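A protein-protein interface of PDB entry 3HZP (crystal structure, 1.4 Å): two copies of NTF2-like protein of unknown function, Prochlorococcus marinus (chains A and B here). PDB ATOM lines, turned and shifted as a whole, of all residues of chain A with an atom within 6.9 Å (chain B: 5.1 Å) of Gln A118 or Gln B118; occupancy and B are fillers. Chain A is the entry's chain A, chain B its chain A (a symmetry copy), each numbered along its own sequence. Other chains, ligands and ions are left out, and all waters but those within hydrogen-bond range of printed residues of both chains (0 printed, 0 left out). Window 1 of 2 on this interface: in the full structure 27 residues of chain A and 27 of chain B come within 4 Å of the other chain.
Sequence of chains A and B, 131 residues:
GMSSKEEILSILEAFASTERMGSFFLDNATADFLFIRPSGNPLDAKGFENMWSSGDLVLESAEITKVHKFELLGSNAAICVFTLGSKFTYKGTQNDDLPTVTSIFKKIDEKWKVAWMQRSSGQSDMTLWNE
Thr A100 touches Gln B118, and with the chains exchanged Gln A118 touches Thr B100. Thr A102 touches Trp B116, and with the chains exchanged Trp A116 touches Thr B102. Thr A102 touches Gln B118, and with the chains exchanged Gln A118 touches Thr B102. Gln B118 touches its own counterpart, Gln A118.
CG2 of Ile A36 touches CG2 of Thr B100, 3.8 Å away. Pro A38 touches Ser B120 (O to CB, 3.3 Å). O of Ser A39 touches OG of Ser B120 (3.6 Å). Gly A40 touches Ser B120. Trp B116 touches Val A81. Thr A100 touches Ile B36 (CG2 to CG2, 3.8 Å). Gln A118 touches Gln B118 (O to OE1, 3.6 Å). Arg B119 touches Gln A118. NE2 of Gln B118 touches C of Arg A119 (3.5 Å).
Of chain A, only Thr A100 (3.3 Å), Thr A102 (2.6 Å), Gln A118 (3.6 Å), Arg A119 (3.5 Å) and Ser A120 (3.4 Å) come within 4 Å of Gln B118. Printed residues of chain B within 4 Å of Ile A36: Thr B100. Of the printed residues of chain A, Arg B119 touches Gln A118. Of the printed residues of chain B, Arg A119 touches Gln B118. Printed residues of chain A within 4 Å of Thr B100: Ile A36, Gly A40 and Gln A118. Of the printed residues of chain B, Gly A40 touches Thr B100 (2.6 Å) and Ser B120 (3.2 Å). Pro A99 touches none of the printed residues of chain B. Val B101 touches none of the printed residues of chain A. The nearest residue of chain B that does not touch Gln A118 is Val B101 (4.1 Å). The nearest residue of chain A that does not touch Gln B118 is Val A101 (4.1 Å).
The backbone NH (N) of Ser A120 lies close to the side-chain amide nitrogen (NE2) of Gln B118. The side-chain amide nitrogen of Gln A118 lies close to the backbone NH of Ser B120, 3.4 Å away. The side-chain hydroxyl (OG1) of Thr B102 is in hydrogen-bond range of the indole nitrogen (NE1) of Trp A116 (2.9 Å). OG1 of Thr B102 is in hydrogen-bond range of OE1 of Gln A118 (2.6 Å). NE1 of Trp B116 lies within hydrogen-bond range of OG1 of Thr A102 (2.9 Å). The side-chain amide nitrogen (NE2) of Gln A118 lies within hydrogen-bond range of the backbone carbonyl oxygen (O) of Thr B100 (3.3 Å). The backbone carbonyl oxygen (O) of Gly A40 sits at hydrogen-bond distance from the side-chain hydroxyl (OG1) of Thr B100 (2.6 Å). OE1 of Gln B118 lies within hydrogen-bond range of OG1 of Thr A102. O of Thr A100 is in hydrogen-bond range of NE2 of Gln B118 (3.3 Å).
Of the 10 printed residues of chain B, 7 touch a printed residue of chain A. Printed residues of chain B that touch a printed residue of chain A: Ile B36, Thr B100, Thr B102, Trp B116, Gln B118, Arg B119 and Ser B120. Hydrophobic or aromatic side chains of chain B that line the printed part of chain A: Ile B36 and Trp B116. Of the 21 printed residues of chain A, 11 touch a printed residue of chain B. Among the printed residues, no Asp or Glu carboxylate lies within 4 Å of a Lys or Arg side-chain nitrogen of the other chain.
The backbone NH (N) of Thr B102 is in hydrogen-bond range of the backbone carbonyl oxygen (O) of Gln B118 (2.9 Å). The backbone NH of Arg B119 sits at hydrogen-bond distance from the backbone carbonyl oxygen of Ile B36 (3.1 Å). The side-chain hydroxyl of Ser A120 lies within hydrogen-bond range of the backbone NH of Thr A100, at 2.9 Å. The backbone carbonyl oxygen (O) of Ile A36 sits at hydrogen-bond distance from the backbone NH (N) of Arg A119 (3.1 Å). The backbone NH (N) of Ile B36 sits at hydrogen-bond distance from the backbone carbonyl oxygen (O) of Met B117 (2.8 Å). The backbone NH (N) of Ile A104 sits at hydrogen-bond distance from the backbone carbonyl oxygen (O) of Trp A116, at 3.0 Å.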
ATOM      1  N   PHE A  33     -13.236 -11.400   5.899  1.00  0.00           N
ATOM      2  CA  PHE A  33     -12.356 -11.353   4.731  1.00  0.00           C
ATOM      3  C   PHE A  33     -12.385  -9.984   4.075  1.00  0.00           C
ATOM      4  O   PHE A  33     -13.437  -9.393   3.902  1.00  0.00           O
ATOM      5  CB  PHE A  33     -12.848 -12.362   3.705  1.00  0.00           C
ATOM      6  CG  PHE A  33     -12.181 -12.233   2.356  1.00  0.00           C
ATOM      7  CD1 PHE A  33     -11.007 -12.871   2.094  1.00  0.00           C
ATOM      8  CD2 PHE A  33     -12.746 -11.480   1.352  1.00  0.00           C
ATOM      9  CE1 PHE A  33     -10.361 -12.729   0.884  1.00  0.00           C
ATOM     10  CE2 PHE A  33     -12.089 -11.332   0.119  1.00  0.00           C
ATOM     11  CZ  PHE A  33     -10.934 -11.964  -0.121  1.00  0.00           C
ATOM     12  N   LEU A  34     -11.204  -9.535   3.647  1.00  0.00           N
ATOM     13  CA  LEU A  34     -11.082  -8.458   2.677  1.00  0.00           C
ATOM     14  C   LEU A  34     -10.057  -8.849   1.626  1.00  0.00           C
ATOM     15  O   LEU A  34      -9.138  -9.618   1.891  1.00  0.00           O
ATOM     16  CB  LEU A  34     -10.673  -7.140   3.327  1.00  0.00           C
ATOM     17  CG  LEU A  34     -11.618  -6.549   4.330  1.00  0.00           C
ATOM     18  CD1 LEU A  34     -10.991  -5.386   5.120  1.00  0.00           C
ATOM     19  CD2 LEU A  34     -12.919  -6.068   3.684  1.00  0.00           C
ATOM     20  N   PHE A  35     -10.237  -8.283   0.445  1.00  0.00           N
ATOM     21  CA  PHE A  35      -9.343  -8.403  -0.697  1.00  0.00           C
ATOM     22  C   PHE A  35      -8.632  -7.075  -0.862  1.00  0.00           C
ATOM     23  O   PHE A  35      -9.298  -6.037  -1.034  1.00  0.00           O
ATOM     24  CB  PHE A  35     -10.176  -8.712  -1.964  1.00  0.00           C
ATOM     25  CG  PHE A  35      -9.375  -8.831  -3.220  1.00  0.00           C
ATOM     26  CD1 PHE A  35      -8.850 -10.044  -3.595  1.00  0.00           C
ATOM     27  CD2 PHE A  35      -9.173  -7.721  -4.033  1.00  0.00           C
ATOM     28  CE1 PHE A  35      -8.107 -10.160  -4.768  1.00  0.00           C
ATOM     29  CE2 PHE A  35      -8.449  -7.848  -5.230  1.00  0.00           C
ATOM     30  CZ  PHE A  35      -7.952  -9.054  -5.572  1.00  0.00           C
ATOM     31  N   ILE A  36      -7.309  -7.073  -0.747  1.00  0.00           N
ATOM     32  CA  ILE A  36      -6.502  -5.852  -0.821  1.00  0.00           C
ATOM     33  C   ILE A  36      -5.987  -5.683  -2.223  1.00  0.00           C
ATOM     34  O   ILE A  36      -5.219  -6.486  -2.712  1.00  0.00           O
ATOM     35  CB  ILE A  36      -5.369  -5.839   0.207  1.00  0.00           C
ATOM     36  CG1 ILE A  36      -5.891  -6.111   1.620  1.00  0.00           C
ATOM     37  CG2 ILE A  36      -4.631  -4.505   0.161  1.00  0.00           C
ATOM     38  CD1 ILE A  36      -7.059  -5.206   2.073  1.00  0.00           C
ATOM     39  N   ARG A  37      -6.495  -4.648  -2.889  1.00  0.00           N
ATOM     40  CA  ARG A  37      -6.098  -4.296  -4.246  1.00  0.00           C
ATOM     41  C   ARG A  37      -4.662  -3.771  -4.292  1.00  0.00           C
ATOM     42  O   ARG A  37      -4.083  -3.395  -3.239  1.00  0.00           O
ATOM     43  CB  ARG A  37      -7.053  -3.251  -4.787  1.00  0.00           C
ATOM     44  CG  ARG A  37      -8.459  -3.770  -4.997  1.00  0.00           C
ATOM     45  CD  ARG A  37      -9.407  -2.628  -5.419  1.00  0.00           C
ATOM     46  NE  ARG A  37      -9.924  -1.953  -4.251  1.00  0.00           N
ATOM     47  CZ  ARG A  37     -10.891  -1.036  -4.271  1.00  0.00           C
ATOM     48  NH1 ARG A  37     -11.382  -0.626  -5.429  1.00  0.00           N
ATOM     49  NH2 ARG A  37     -11.356  -0.538  -3.125  1.00  0.00           N
ATOM     50  N   PRO A  38      -4.083  -3.682  -5.494  1.00  0.00           N
ATOM     51  CA  PRO A  38      -2.717  -3.176  -5.598  1.00  0.00           C
ATOM     52  C   PRO A  38      -2.529  -1.789  -4.989  1.00  0.00           C
ATOM     53  O   PRO A  38      -1.427  -1.482  -4.501  1.00  0.00           O
ATOM     54  CB  PRO A  38      -2.479  -3.142  -7.114  1.00  0.00           C
ATOM     55  CG  PRO A  38      -3.309  -4.290  -7.622  1.00  0.00           C
ATOM     56  CD  PRO A  38      -4.559  -4.163  -6.807  1.00  0.00           C
ATOM     57  N   SER A  39      -3.555  -0.937  -5.018  1.00  0.00           N
ATOM     58  CA  SER A  39      -3.545   0.344  -4.376  1.00  0.00           C
ATOM     59  C   SER A  39      -3.471   0.310  -2.855  1.00  0.00           C
ATOM     60  O   SER A  39      -3.193   1.351  -2.238  1.00  0.00           O
ATOM     61  CB  SER A  39      -4.845   1.045  -4.736  1.00  0.00           C
ATOM     62  OG  SER A  39      -5.931   0.277  -4.266  1.00  0.00           O
ATOM     63  N   GLY A  40      -3.773  -0.840  -2.266  1.00  0.00           N
ATOM     64  CA  GLY A  40      -3.945  -0.956  -0.831  1.00  0.00           C
ATOM     65  C   GLY A  40      -5.384  -0.837  -0.376  1.00  0.00           C
ATOM     66  O   GLY A  40      -5.703  -1.017   0.791  1.00  0.00           O
ATOM     67  N   VAL A  81       1.085 -18.429  -0.693  1.00  0.00           N
ATOM     68  CA  VAL A  81       1.541 -17.365  -1.565  1.00  0.00           C
ATOM     69  C   VAL A  81       1.712 -17.917  -2.948  1.00  0.00           C
ATOM     70  O   VAL A  81       2.351 -18.960  -3.108  1.00  0.00           O
ATOM     71  CB  VAL A  81       2.881 -16.763  -1.056  1.00  0.00           C
ATOM     72  CG1 VAL A  81       3.410 -15.681  -2.038  1.00  0.00           C
ATOM     73  CG2 VAL A  81       2.727 -16.205   0.388  1.00  0.00           C
ATOM     74  N   PRO A  99       0.041 -11.052 -10.962  1.00  0.00           N
ATOM     75  CA  PRO A  99       0.416 -10.584  -9.616  1.00  0.00           C
ATOM     76  C   PRO A  99       0.989 -11.709  -8.737  1.00  0.00           C
ATOM     77  O   PRO A  99       0.721 -12.911  -8.923  1.00  0.00           O
ATOM     78  CB  PRO A  99      -0.897 -10.135  -9.017  1.00  0.00           C
ATOM     79  CG  PRO A  99      -1.911 -11.045  -9.679  1.00  0.00           C
ATOM     80  CD  PRO A  99      -1.415 -11.199 -11.063  1.00  0.00           C
ATOM     81  N   THR A 100       1.686 -11.277  -7.700  1.00  0.00           N
ATOM     82  CA  THR A 100       1.920 -12.062  -6.492  1.00  0.00           C
ATOM     83  C   THR A 100       0.775 -11.853  -5.513  1.00  0.00           C
ATOM     84  O   THR A 100       0.361 -10.702  -5.264  1.00  0.00           O
ATOM     85  CB  THR A 100       3.218 -11.619  -5.794  1.00  0.00           C
ATOM     86  OG1 THR A 100       4.314 -11.843  -6.692  1.00  0.00           O
ATOM     87  CG2 THR A 100       3.472 -12.406  -4.476  1.00  0.00           C
ATOM     88  N   VAL A 101       0.259 -12.966  -4.994  1.00  0.00           N
ATOM     89  CA  VAL A 101      -0.855 -12.956  -4.066  1.00  0.00           C
ATOM     90  C   VAL A 101      -0.529 -13.664  -2.774  1.00  0.00           C
ATOM     91  O   VAL A 101      -0.018 -14.788  -2.796  1.00  0.00           O
ATOM     92  CB  VAL A 101      -2.087 -13.665  -4.704  1.00  0.00           C
ATOM     93  CG1 VAL A 101      -3.270 -13.594  -3.791  1.00  0.00           C
ATOM     94  CG2 VAL A 101      -2.375 -13.080  -6.098  1.00  0.00           C
ATOM     95  N   THR A 102      -0.761 -12.992  -1.648  1.00  0.00           N
ATOM     96  CA  THR A 102      -0.651 -13.585  -0.309  1.00  0.00           C
ATOM     97  C   THR A 102      -2.062 -13.882   0.151  1.00  0.00           C
ATOM     98  O   THR A 102      -2.911 -12.976   0.209  1.00  0.00           O
ATOM     99  CB  THR A 102       0.024 -12.644   0.669  1.00  0.00           C
ATOM    100  OG1 THR A 102       1.362 -12.401   0.258  1.00  0.00           O
ATOM    101  CG2 THR A 102      -0.004 -13.223   2.096  1.00  0.00           C
ATOM    102  N   SER A 103      -2.354 -15.153   0.427  1.00  0.00           N
ATOM    103  CA  SER A 103      -3.682 -15.564   0.912  1.00  0.00           C
ATOM    104  C   SER A 103      -3.536 -16.249   2.249  1.00  0.00           C
ATOM    105  O   SER A 103      -2.531 -16.943   2.501  1.00  0.00           O
ATOM    106  CB  SER A 103      -4.382 -16.447  -0.108  1.00  0.00           C
ATOM    107  OG  SER A 103      -3.736 -17.735  -0.287  1.00  0.00           O
ATOM    108  N   ILE A 104      -4.528 -16.075   3.108  1.00  0.00           N
ATOM    109  CA  ILE A 104      -4.584 -16.705   4.409  1.00  0.00           C
ATOM    110  C   ILE A 104      -5.922 -17.444   4.493  1.00  0.00           C
ATOM    111  O   ILE A 104      -6.938 -16.940   3.995  1.00  0.00           O
ATOM    112  CB  ILE A 104      -4.489 -15.693   5.542  1.00  0.00           C
ATOM    113  CG1 ILE A 104      -3.247 -14.819   5.382  1.00  0.00           C
ATOM    114  CG2 ILE A 104      -4.615 -16.362   6.886  1.00  0.00           C
ATOM    115  CD1 ILE A 104      -2.000 -15.583   5.470  1.00  0.00           C
ATOM    116  N   TRP A 116      -8.223 -13.978   4.002  1.00  0.00           N
ATOM    117  CA  TRP A 116      -7.531 -12.725   3.642  1.00  0.00           C
ATOM    118  C   TRP A 116      -6.843 -12.931   2.317  1.00  0.00           C
ATOM    119  O   TRP A 116      -6.333 -14.004   2.017  1.00  0.00           O
ATOM    120  CB  TRP A 116      -6.489 -12.337   4.692  1.00  0.00           C
ATOM    121  CG  TRP A 116      -6.027 -10.967   4.558  1.00  0.00           C
ATOM    122  CD1 TRP A 116      -4.841 -10.545   4.026  1.00  0.00           C
ATOM    123  CD2 TRP A 116      -6.717  -9.793   4.985  1.00  0.00           C
ATOM    124  NE1 TRP A 116      -4.777  -9.169   4.058  1.00  0.00           N
ATOM    125  CE2 TRP A 116      -5.905  -8.680   4.637  1.00  0.00           C
ATOM    126  CE3 TRP A 116      -7.935  -9.571   5.615  1.00  0.00           C
ATOM    127  CZ2 TRP A 116      -6.284  -7.390   4.902  1.00  0.00           C
ATOM    128  CZ3 TRP A 116      -8.311  -8.268   5.894  1.00  0.00           C
ATOM    129  CH2 TRP A 116      -7.468  -7.200   5.538  1.00  0.00           C
ATOM    130  N   MET A 117      -6.787 -11.894   1.498  1.00  0.00           N
ATOM    131  CA  MET A 117      -6.010 -11.948   0.261  1.00  0.00           C
ATOM    132  C   MET A 117      -5.534 -10.535  -0.123  1.00  0.00           C
ATOM    133  O   MET A 117      -6.352  -9.623  -0.171  1.00  0.00           O
ATOM    134  CB  MET A 117      -6.839 -12.529  -0.875  1.00  0.00           C
ATOM    135  CG  MET A 117      -6.093 -12.658  -2.203  1.00  0.00           C
ATOM    136  SD  MET A 117      -7.114 -13.496  -3.627  1.00  0.00           S
ATOM    137  CE  MET A 117      -7.139 -15.288  -2.830  1.00  0.00           C
ATOM    138  N   GLN A 118      -4.233 -10.399  -0.391  1.00  0.00           N
ATOM    139  CA  GLN A 118      -3.658  -9.182  -0.920  1.00  0.00           C
ATOM    140  C   GLN A 118      -2.925  -9.511  -2.196  1.00  0.00           C
ATOM    141  O   GLN A 118      -2.134 -10.453  -2.245  1.00  0.00           O
ATOM    142  CB  GLN A 118      -2.706  -8.529   0.103  1.00  0.00           C
ATOM    143  CG  GLN A 118      -2.019  -7.254  -0.423  1.00  0.00           C
ATOM    144  CD  GLN A 118      -1.447  -6.335   0.626  1.00  0.00           C
ATOM    145  OE1 GLN A 118      -1.602  -6.573   1.827  1.00  0.00           O
ATOM    146  NE2 GLN A 118      -0.839  -5.250   0.195  1.00  0.00           N
ATOM    147  N   ARG A 119      -3.152  -8.704  -3.218  1.00  0.00           N
ATOM    148  CA  ARG A 119      -2.480  -8.854  -4.496  1.00  0.00           C
ATOM    149  C   ARG A 119      -1.637  -7.658  -4.872  1.00  0.00           C
ATOM    150  O   ARG A 119      -1.954  -6.523  -4.525  1.00  0.00           O
ATOM    151  CB  ARG A 119      -3.454  -9.149  -5.646  1.00  0.00           C
ATOM    152  CG  ARG A 119      -4.445  -8.051  -5.956  1.00  0.00           C
ATOM    153  CD  ARG A 119      -4.984  -8.151  -7.384  1.00  0.00           C
ATOM    154  NE  ARG A 119      -3.969  -7.785  -8.343  1.00  0.00           N
ATOM    155  CZ  ARG A 119      -4.004  -8.055  -9.639  1.00  0.00           C
ATOM    156  NH1 ARG A 119      -5.040  -8.686 -10.165  1.00  0.00           N
ATOM    157  NH2 ARG A 119      -3.000  -7.694 -10.410  1.00  0.00           N
ATOM    158  N   SER A 120      -0.603  -7.924  -5.660  1.00  0.00           N
ATOM    159  CA  SER A 120       0.284  -6.898  -6.178  1.00  0.00           C
ATOM    160  C   SER A 120      -0.233  -6.382  -7.523  1.00  0.00           C
ATOM    161  O   SER A 120      -1.209  -6.890  -8.053  1.00  0.00           O
ATOM    162  CB  SER A 120       1.703  -7.443  -6.358  1.00  0.00           C
ATOM    163  OG  SER A 120       1.782  -8.372  -7.452  1.00  0.00           O
ATOM    164  N   SER A 121       0.488  -5.436  -8.104  1.00  0.00           N
ATOM    165  CA  SER A 121       0.296  -5.121  -9.507  1.00  0.00           C
ATOM    166  C   SER A 121       0.578  -6.380 -10.362  1.00  0.00           C
ATOM    167  O   SER A 121       1.179  -7.391  -9.926  1.00  0.00           O
ATOM    168  CB  SER A 121       1.161  -3.907  -9.882  1.00  0.00           C
ATOM    169  OG  SER A 121       0.685  -2.715  -9.249  1.00  0.00           O
ATOM    170  N   ILE B  36       7.261  -8.552  -0.075  1.00  0.00           N
ATOM    171  CA  ILE B  36       6.655  -8.435  -1.404  1.00  0.00           C
ATOM    172  C   ILE B  36       6.382  -6.986  -1.697  1.00  0.00           C
ATOM    173  O   ILE B  36       5.590  -6.348  -1.035  1.00  0.00           O
ATOM    174  CB  ILE B  36       5.395  -9.292  -1.547  1.00  0.00           C
ATOM    175  CG1 ILE B  36       5.659 -10.746  -1.150  1.00  0.00           C
ATOM    176  CG2 ILE B  36       4.869  -9.218  -2.977  1.00  0.00           C
ATOM    177  CD1 ILE B  36       6.862 -11.411  -1.855  1.00  0.00           C
ATOM    178  N   ARG B  37       7.124  -6.458  -2.669  1.00  0.00           N
ATOM    179  CA  ARG B  37       6.986  -5.081  -3.125  1.00  0.00           C
ATOM    180  C   ARG B  37       5.662  -4.864  -3.858  1.00  0.00           C
ATOM    181  O   ARG B  37       4.992  -5.843  -4.277  1.00  0.00           O
ATOM    182  CB  ARG B  37       8.150  -4.741  -4.036  1.00  0.00           C
ATOM    183  CG  ARG B  37       9.483  -4.703  -3.323  1.00  0.00           C
ATOM    184  CD  ARG B  37      10.635  -4.485  -4.325  1.00  0.00           C
ATOM    185  NE  ARG B  37      11.063  -5.751  -4.875  1.00  0.00           N
ATOM    186  CZ  ARG B  37      12.142  -5.921  -5.638  1.00  0.00           C
ATOM    187  NH1 ARG B  37      12.852  -4.869  -6.012  1.00  0.00           N
ATOM    188  NH2 ARG B  37      12.498  -7.148  -6.020  1.00  0.00           N
ATOM    189  N   THR B 100      -1.108  -0.169   2.497  1.00  0.00           N
ATOM    190  CA  THR B 100      -1.626  -1.284   3.281  1.00  0.00           C
ATOM    191  C   THR B 100      -0.621  -2.426   3.281  1.00  0.00           C
ATOM    192  O   THR B 100      -0.089  -2.796   2.213  1.00  0.00           O
ATOM    193  CB  THR B 100      -2.938  -1.817   2.676  1.00  0.00           C
ATOM    194  OG1 THR B 100      -3.909  -0.761   2.704  1.00  0.00           O
ATOM    195  CG2 THR B 100      -3.492  -3.038   3.464  1.00  0.00           C
ATOM    196  N   VAL B 101      -0.350  -2.947   4.476  1.00  0.00           N
ATOM    197  CA  VAL B 101       0.605  -4.023   4.664  1.00  0.00           C
ATOM    198  C   VAL B 101      -0.006  -5.213   5.362  1.00  0.00           C
ATOM    199  O   VAL B 101      -0.662  -5.055   6.396  1.00  0.00           O
ATOM    200  CB  VAL B 101       1.805  -3.526   5.524  1.00  0.00           C
ATOM    201  CG1 VAL B 101       2.837  -4.599   5.662  1.00  0.00           C
ATOM    202  CG2 VAL B 101       2.376  -2.223   4.938  1.00  0.00           C
ATOM    203  N   THR B 102       0.149  -6.397   4.773  1.00  0.00           N
ATOM    204  CA  THR B 102      -0.241  -7.672   5.391  1.00  0.00           C
ATOM    205  C   THR B 102       1.031  -8.309   5.910  1.00  0.00           C
ATOM    206  O   THR B 102       1.981  -8.538   5.142  1.00  0.00           O
ATOM    207  CB  THR B 102      -0.913  -8.596   4.396  1.00  0.00           C
ATOM    208  OG1 THR B 102      -2.128  -8.015   3.943  1.00  0.00           O
ATOM    209  CG2 THR B 102      -1.179  -9.977   5.025  1.00  0.00           C
ATOM    210  N   TRP B 116       6.477 -12.979   7.056  1.00  0.00           N
ATOM    211  CA  TRP B 116       6.030 -12.597   5.703  1.00  0.00           C
ATOM    212  C   TRP B 116       5.523 -11.179   5.757  1.00  0.00           C
ATOM    213  O   TRP B 116       4.918 -10.748   6.731  1.00  0.00           O
ATOM    214  CB  TRP B 116       4.909 -13.510   5.202  1.00  0.00           C
ATOM    215  CG  TRP B 116       4.671 -13.390   3.775  1.00  0.00           C
ATOM    216  CD1 TRP B 116       3.648 -12.722   3.163  1.00  0.00           C
ATOM    217  CD2 TRP B 116       5.449 -13.977   2.733  1.00  0.00           C
ATOM    218  NE1 TRP B 116       3.776 -12.823   1.795  1.00  0.00           N
ATOM    219  CE2 TRP B 116       4.862 -13.583   1.500  1.00  0.00           C
ATOM    220  CE3 TRP B 116       6.579 -14.785   2.716  1.00  0.00           C
ATOM    221  CZ2 TRP B 116       5.376 -13.972   0.291  1.00  0.00           C
ATOM    222  CZ3 TRP B 116       7.089 -15.188   1.494  1.00  0.00           C
ATOM    223  CH2 TRP B 116       6.469 -14.779   0.301  1.00  0.00           C
ATOM    224  N   MET B 117       5.737 -10.421   4.694  1.00  0.00           N
ATOM    225  CA  MET B 117       5.152  -9.085   4.587  1.00  0.00           C
ATOM    226  C   MET B 117       4.942  -8.719   3.107  1.00  0.00           C
ATOM    227  O   MET B 117       5.879  -8.840   2.325  1.00  0.00           O
ATOM    228  CB  MET B 117       6.049  -8.046   5.243  1.00  0.00           C
ATOM    229  CG  MET B 117       5.497  -6.622   5.212  1.00  0.00           C
ATOM    230  SD  MET B 117       6.590  -5.310   6.140  1.00  0.00           S
ATOM    231  CE  MET B 117       6.243  -5.999   7.944  1.00  0.00           C
ATOM    232  N   GLN B 118       3.728  -8.278   2.770  1.00  0.00           N
ATOM    233  CA  GLN B 118       3.415  -7.744   1.462  1.00  0.00           C
ATOM    234  C   GLN B 118       2.841  -6.360   1.633  1.00  0.00           C
ATOM    235  O   GLN B 118       1.941  -6.146   2.445  1.00  0.00           O
ATOM    236  CB  GLN B 118       2.424  -8.659   0.713  1.00  0.00           C
ATOM    237  CG  GLN B 118       2.010  -8.114  -0.667  1.00  0.00           C
ATOM    238  CD  GLN B 118       1.425  -9.123  -1.623  1.00  0.00           C
ATOM    239  OE1 GLN B 118       1.365 -10.318  -1.321  1.00  0.00           O
ATOM    240  NE2 GLN B 118       1.046  -8.673  -2.801  1.00  0.00           N
ATOM    241  N   ARG B 119       3.328  -5.429   0.832  1.00  0.00           N
ATOM    242  CA  ARG B 119       2.838  -4.062   0.835  1.00  0.00           C
ATOM    243  C   ARG B 119       2.238  -3.641  -0.485  1.00  0.00           C
ATOM    244  O   ARG B 119       2.657  -4.093  -1.547  1.00  0.00           O
ATOM    245  CB  ARG B 119       3.920  -3.047   1.229  1.00  0.00           C
ATOM    246  CG  ARG B 119       5.092  -2.943   0.280  1.00  0.00           C
ATOM    247  CD  ARG B 119       5.817  -1.603   0.407  1.00  0.00           C
ATOM    248  NE  ARG B 119       5.017  -0.532  -0.140  1.00  0.00           N
ATOM    249  CZ  ARG B 119       5.205   0.759   0.085  1.00  0.00           C
ATOM    250  NH1 ARG B 119       6.207   1.169   0.843  1.00  0.00           N
ATOM    251  NH2 ARG B 119       4.387   1.643  -0.448  1.00  0.00           N
ATOM    252  N   SER B 120       1.304  -2.700  -0.404  1.00  0.00           N
ATOM    253  CA  SER B 120       0.658  -2.122  -1.569  1.00  0.00           C
ATOM    254  C   SER B 120       1.436  -0.895  -2.050  1.00  0.00           C
ATOM    255  O   SER B 120       2.398  -0.480  -1.422  1.00  0.00           O
ATOM    256  CB  SER B 120      -0.781  -1.712  -1.247  1.00  0.00           C
ATOM    257  OG  SER B 120      -0.827  -0.566  -0.379  1.00  0.00           O
